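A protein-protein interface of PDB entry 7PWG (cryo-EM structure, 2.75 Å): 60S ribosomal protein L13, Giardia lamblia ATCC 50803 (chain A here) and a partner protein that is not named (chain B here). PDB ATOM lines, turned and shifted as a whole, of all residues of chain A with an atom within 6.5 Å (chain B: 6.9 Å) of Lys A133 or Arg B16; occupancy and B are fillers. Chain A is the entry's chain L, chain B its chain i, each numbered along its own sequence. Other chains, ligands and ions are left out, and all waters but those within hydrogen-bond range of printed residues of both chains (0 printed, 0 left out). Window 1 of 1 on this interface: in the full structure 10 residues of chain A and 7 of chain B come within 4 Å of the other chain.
The backbone NH (N) of Val B15 sits at hydrogen-bond distance from the side-chain carboxylate (OE2) of Glu A136 (3.4 Å).
The backbone carbonyl oxygen (O) of Lys A133 is in hydrogen-bond range of the backbone NH (N) of Ile B17 (3.3 Å).
O of Val B15 lies within hydrogen-bond range of N of Glu A135 (3.0 Å).
The side-chain hydroxyl (OG) of Ser A134 lies within hydrogen-bond range of the side-chain hydroxyl (OG) of Ser A137 (2.8 Å).
O of Lys A131 lies within hydrogen-bond range of NZ of Lys A133 (2.8 Å).
Among the printed residues, merely in contact across the chains: Asn A132 with Ile B17 (3.8 Å), Lys A133 with Arg B16 (3.7 Å), Ser A134 with Val B15 (3.2 Å), Ser A134 with Ile B17 (3.3 Å), Glu A135 with Ile B17 (3.6 Å) and Glu A136 with Val B14 (3.2 Å).
Of chain B, only Arg B16 and Ile B17 come within 4 Å of Lys A133.
Of chain A, only Lys A133 comes within 4 Å of Arg B16.
Of the printed residues of chain B, Glu A135 touches Val B15 and Ile B17.
Printed residues of chain A within 4 Å of Val B14: Glu A136.
Printed residues of chain B within 4 Å of Ser A134: Val B15 (3.2 Å) and Ile B17 (3.3 Å).
Gly B12 touches none of the printed residues of chain A.
The nearest residue of chain B that does not touch Lys A133 is Val B15 (4.5 Å).
Of the 8 printed residues of chain A, 5 touch a printed residue of chain B.
Printed residues of chain B that touch a printed residue of chain A: Val B14, Val B15, Arg B16 and Ile B17.
Hydrophobic or aromatic side chains of chain B that line the printed part of chain A: Val B14 and Ile B17.
Among the printed residues, no Asp or Glu carboxylate lies within 4 Å of a Lys or Arg side-chain nitrogen of the other chain.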
ATOM      1  N   ARG A 130     -10.880 -22.901  -4.699  1.00  0.00           N
ATOM      2  CA  ARG A 130     -10.558 -23.062  -6.112  1.00  0.00           C
ATOM      3  C   ARG A 130     -11.469 -22.222  -6.997  1.00  0.00           C
ATOM      4  O   ARG A 130     -12.664 -22.090  -6.736  1.00  0.00           O
ATOM      5  CB  ARG A 130     -10.664 -24.532  -6.526  1.00  0.00           C
ATOM      6  CG  ARG A 130     -10.533 -24.775  -8.012  1.00  0.00           C
ATOM      7  CD  ARG A 130     -10.072 -26.180  -8.346  1.00  0.00           C
ATOM      8  NE  ARG A 130     -11.165 -27.135  -8.426  1.00  0.00           N
ATOM      9  CZ  ARG A 130     -11.921 -27.332  -9.500  1.00  0.00           C
ATOM     10  NH1 ARG A 130     -12.876 -28.234  -9.462  1.00  0.00           N
ATOM     11  NH2 ARG A 130     -11.727 -26.631 -10.603  1.00  0.00           N
ATOM     12  N   LYS A 131     -10.892 -21.675  -8.064  1.00  0.00           N
ATOM     13  CA  LYS A 131     -11.596 -20.901  -9.079  1.00  0.00           C
ATOM     14  C   LYS A 131     -11.331 -21.505 -10.448  1.00  0.00           C
ATOM     15  O   LYS A 131     -10.208 -21.921 -10.733  1.00  0.00           O
ATOM     16  CB  LYS A 131     -11.150 -19.446  -9.073  1.00  0.00           C
ATOM     17  CG  LYS A 131     -11.456 -18.757  -7.794  1.00  0.00           C
ATOM     18  CD  LYS A 131     -12.909 -18.950  -7.446  1.00  0.00           C
ATOM     19  CE  LYS A 131     -13.196 -18.517  -6.033  1.00  0.00           C
ATOM     20  NZ  LYS A 131     -12.810 -17.111  -5.833  1.00  0.00           N
ATOM     21  N   ASN A 132     -12.358 -21.552 -11.291  1.00  0.00           N
ATOM     22  CA  ASN A 132     -12.184 -22.107 -12.625  1.00  0.00           C
ATOM     23  C   ASN A 132     -11.385 -21.153 -13.501  1.00  0.00           C
ATOM     24  O   ASN A 132     -11.470 -19.931 -13.373  1.00  0.00           O
ATOM     25  CB  ASN A 132     -13.534 -22.415 -13.271  1.00  0.00           C
ATOM     26  CG  ASN A 132     -14.252 -23.568 -12.597  1.00  0.00           C
ATOM     27  OD1 ASN A 132     -15.120 -23.365 -11.755  1.00  0.00           O
ATOM     28  ND2 ASN A 132     -13.894 -24.781 -12.968  1.00  0.00           N
ATOM     29  N   LYS A 133     -10.575 -21.726 -14.380  1.00  0.00           N
ATOM     30  CA  LYS A 133      -9.754 -20.937 -15.280  1.00  0.00           C
ATOM     31  C   LYS A 133     -10.336 -20.838 -16.678  1.00  0.00           C
ATOM     32  O   LYS A 133      -9.846 -20.039 -17.474  1.00  0.00           O
ATOM     33  CB  LYS A 133      -8.338 -21.519 -15.354  1.00  0.00           C
ATOM     34  CG  LYS A 133      -7.676 -21.767 -14.004  1.00  0.00           C
ATOM     35  CD  LYS A 133      -7.431 -20.476 -13.247  1.00  0.00           C
ATOM     36  CE  LYS A 133      -6.664 -20.701 -11.961  1.00  0.00           C
ATOM     37  NZ  LYS A 133      -7.515 -21.010 -10.797  1.00  0.00           N
ATOM     38  N   SER A 134     -11.366 -21.614 -16.996  1.00  0.00           N
ATOM     39  CA  SER A 134     -11.909 -21.627 -18.345  1.00  0.00           C
ATOM     40  C   SER A 134     -13.305 -22.230 -18.332  1.00  0.00           C
ATOM     41  O   SER A 134     -13.778 -22.744 -17.318  1.00  0.00           O
ATOM     42  CB  SER A 134     -11.004 -22.402 -19.300  1.00  0.00           C
ATOM     43  OG  SER A 134     -10.904 -23.754 -18.908  1.00  0.00           O
ATOM     44  N   GLU A 135     -13.953 -22.159 -19.489  1.00  0.00           N
ATOM     45  CA  GLU A 135     -15.292 -22.705 -19.656  1.00  0.00           C
ATOM     46  C   GLU A 135     -15.295 -24.218 -19.788  1.00  0.00           C
ATOM     47  O   GLU A 135     -16.265 -24.859 -19.380  1.00  0.00           O
ATOM     48  CB  GLU A 135     -15.961 -22.076 -20.873  1.00  0.00           C
ATOM     49  CG  GLU A 135     -16.529 -20.731 -20.582  1.00  0.00           C
ATOM     50  CD  GLU A 135     -17.522 -20.780 -19.446  1.00  0.00           C
ATOM     51  OE1 GLU A 135     -18.568 -21.440 -19.601  1.00  0.00           O
ATOM     52  OE2 GLU A 135     -17.258 -20.168 -18.390  1.00  0.00           O
ATOM     53  N   GLU A 136     -14.234 -24.805 -20.340  1.00  0.00           N
ATOM     54  CA  GLU A 136     -14.164 -26.260 -20.416  1.00  0.00           C
ATOM     55  C   GLU A 136     -13.995 -26.899 -19.049  1.00  0.00           C
ATOM     56  O   GLU A 136     -14.482 -28.013 -18.833  1.00  0.00           O
ATOM     57  CB  GLU A 136     -13.029 -26.698 -21.331  1.00  0.00           C
ATOM     58  CG  GLU A 136     -13.360 -26.629 -22.802  1.00  0.00           C
ATOM     59  CD  GLU A 136     -13.466 -25.208 -23.317  1.00  0.00           C
ATOM     60  OE1 GLU A 136     -14.125 -25.003 -24.351  1.00  0.00           O
ATOM     61  OE2 GLU A 136     -12.892 -24.298 -22.687  1.00  0.00           O
ATOM     62  N   SER A 137     -13.311 -26.230 -18.120  1.00  0.00           N
ATOM     63  CA  SER A 137     -13.152 -26.792 -16.785  1.00  0.00           C
ATOM     64  C   SER A 137     -14.492 -27.017 -16.113  1.00  0.00           C
ATOM     65  O   SER A 137     -14.618 -27.906 -15.268  1.00  0.00           O
ATOM     66  CB  SER A 137     -12.296 -25.879 -15.916  1.00  0.00           C
ATOM     67  OG  SER A 137     -11.213 -25.358 -16.651  1.00  0.00           O
ATOM     68  N   LYS B  10      -1.126 -19.771 -28.618  1.00  0.00           N
ATOM     69  CA  LYS B  10      -1.263 -20.059 -27.197  1.00  0.00           C
ATOM     70  C   LYS B  10      -2.616 -19.576 -26.693  1.00  0.00           C
ATOM     71  O   LYS B  10      -3.007 -18.429 -26.927  1.00  0.00           O
ATOM     72  CB  LYS B  10      -0.144 -19.404 -26.389  1.00  0.00           C
ATOM     73  CG  LYS B  10      -0.195 -19.742 -24.906  1.00  0.00           C
ATOM     74  CD  LYS B  10       0.633 -18.776 -24.067  1.00  0.00           C
ATOM     75  CE  LYS B  10       2.114 -19.124 -24.088  1.00  0.00           C
ATOM     76  NZ  LYS B  10       2.401 -20.354 -23.329  1.00  0.00           N
ATOM     77  N   GLY B  11      -3.314 -20.447 -25.973  1.00  0.00           N
ATOM     78  CA  GLY B  11      -4.657 -20.167 -25.521  1.00  0.00           C
ATOM     79  C   GLY B  11      -5.737 -20.414 -26.543  1.00  0.00           C
ATOM     80  O   GLY B  11      -6.872 -19.986 -26.331  1.00  0.00           O
ATOM     81  N   GLY B  12      -5.427 -21.096 -27.641  1.00  0.00           N
ATOM     82  CA  GLY B  12      -6.359 -21.250 -28.734  1.00  0.00           C
ATOM     83  C   GLY B  12      -7.346 -22.383 -28.608  1.00  0.00           C
ATOM     84  O   GLY B  12      -8.234 -22.494 -29.454  1.00  0.00           O
ATOM     85  N   VAL B  14      -9.142 -23.294 -25.448  1.00  0.00           N
ATOM     86  CA  VAL B  14     -10.182 -23.083 -24.453  1.00  0.00           C
ATOM     87  C   VAL B  14     -10.566 -21.607 -24.440  1.00  0.00           C
ATOM     88  O   VAL B  14      -9.896 -20.764 -25.028  1.00  0.00           O
ATOM     89  CB  VAL B  14      -9.751 -23.546 -23.045  1.00  0.00           C
ATOM     90  CG1 VAL B  14      -9.353 -25.019 -23.056  1.00  0.00           C
ATOM     91  CG2 VAL B  14      -8.615 -22.676 -22.511  1.00  0.00           C
ATOM     92  N   VAL B  15     -11.669 -21.312 -23.764  1.00  0.00           N
ATOM     93  CA  VAL B  15     -12.153 -19.952 -23.558  1.00  0.00           C
ATOM     94  C   VAL B  15     -11.897 -19.587 -22.104  1.00  0.00           C
ATOM     95  O   VAL B  15     -12.432 -20.234 -21.199  1.00  0.00           O
ATOM     96  CB  VAL B  15     -13.645 -19.823 -23.898  1.00  0.00           C
ATOM     97  CG1 VAL B  15     -14.140 -18.425 -23.599  1.00  0.00           C
ATOM     98  CG2 VAL B  15     -13.882 -20.172 -25.338  1.00  0.00           C
ATOM     99  N   ARG B  16     -11.091 -18.556 -21.876  1.00  0.00           N
ATOM    100  CA  ARG B  16     -10.732 -18.188 -20.515  1.00  0.00           C
ATOM    101  C   ARG B  16     -11.922 -17.570 -19.791  1.00  0.00           C
ATOM    102  O   ARG B  16     -12.903 -17.149 -20.402  1.00  0.00           O
ATOM    103  CB  ARG B  16      -9.542 -17.225 -20.504  1.00  0.00           C
ATOM    104  CG  ARG B  16      -8.222 -17.925 -20.230  1.00  0.00           C
ATOM    105  CD  ARG B  16      -6.979 -17.037 -20.413  1.00  0.00           C
ATOM    106  NE  ARG B  16      -5.787 -17.876 -20.546  1.00  0.00           N
ATOM    107  CZ  ARG B  16      -5.409 -18.452 -21.685  1.00  0.00           C
ATOM    108  NH1 ARG B  16      -6.112 -18.253 -22.792  1.00  0.00           N
ATOM    109  NH2 ARG B  16      -4.330 -19.217 -21.731  1.00  0.00           N
ATOM    110  N   ILE B  17     -11.838 -17.553 -18.464  1.00  0.00           N
ATOM    111  CA  ILE B  17     -12.816 -16.882 -17.615  1.00  0.00           C
ATOM    112  C   ILE B  17     -12.158 -15.629 -17.061  1.00  0.00           C
ATOM    113  O   ILE B  17     -11.174 -15.714 -16.316  1.00  0.00           O
ATOM    114  CB  ILE B  17     -13.311 -17.781 -16.472  1.00  0.00           C
ATOM    115  CG1 ILE B  17     -14.040 -19.016 -16.986  1.00  0.00           C
ATOM    116  CG2 ILE B  17     -14.222 -17.004 -15.561  1.00  0.00           C
ATOM    117  CD1 ILE B  17     -14.629 -19.853 -15.899  1.00  0.00           C
ATOM    118  N   VAL B  18     -12.693 -14.467 -17.411  1.00  0.00           N
ATOM    119  CA  VAL B  18     -12.162 -13.204 -16.911  1.00  0.00           C
ATOM    120  C   VAL B  18     -12.954 -12.820 -15.665  1.00  0.00           C
ATOM    121  O   VAL B  18     -14.137 -12.482 -15.738  1.00  0.00           O
ATOM    122  CB  VAL B  18     -12.202 -12.107 -17.983  1.00  0.00           C
ATOM    123  CG1 VAL B  18     -11.078 -12.327 -18.991  1.00  0.00           C
ATOM    124  CG2 VAL B  18     -13.548 -12.087 -18.701  1.00  0.00           C
ATOM    125  N   ARG B  19     -12.305 -12.914 -14.514  1.00  0.00           N
ATOM    126  CA  ARG B  19     -12.941 -12.623 -13.242  1.00  0.00           C
ATOM    127  C   ARG B  19     -12.935 -11.121 -12.980  1.00  0.00           C
ATOM    128  O   ARG B  19     -12.041 -10.397 -13.424  1.00  0.00           O
ATOM    129  CB  ARG B  19     -12.221 -13.373 -12.123  1.00  0.00           C
ATOM    130  CG  ARG B  19     -10.738 -13.559 -12.395  1.00  0.00           C
ATOM    131  CD  ARG B  19     -10.072 -14.506 -11.396  1.00  0.00           C
ATOM    132  NE  ARG B  19     -10.296 -14.086 -10.018  1.00  0.00           N
ATOM    133  CZ  ARG B  19      -9.717 -14.645  -8.962  1.00  0.00           C
ATOM    134  NH1 ARG B  19      -8.872 -15.656  -9.117  1.00  0.00           N
ATOM    135  NH2 ARG B  19      -9.990 -14.195  -7.746  1.00  0.00           N
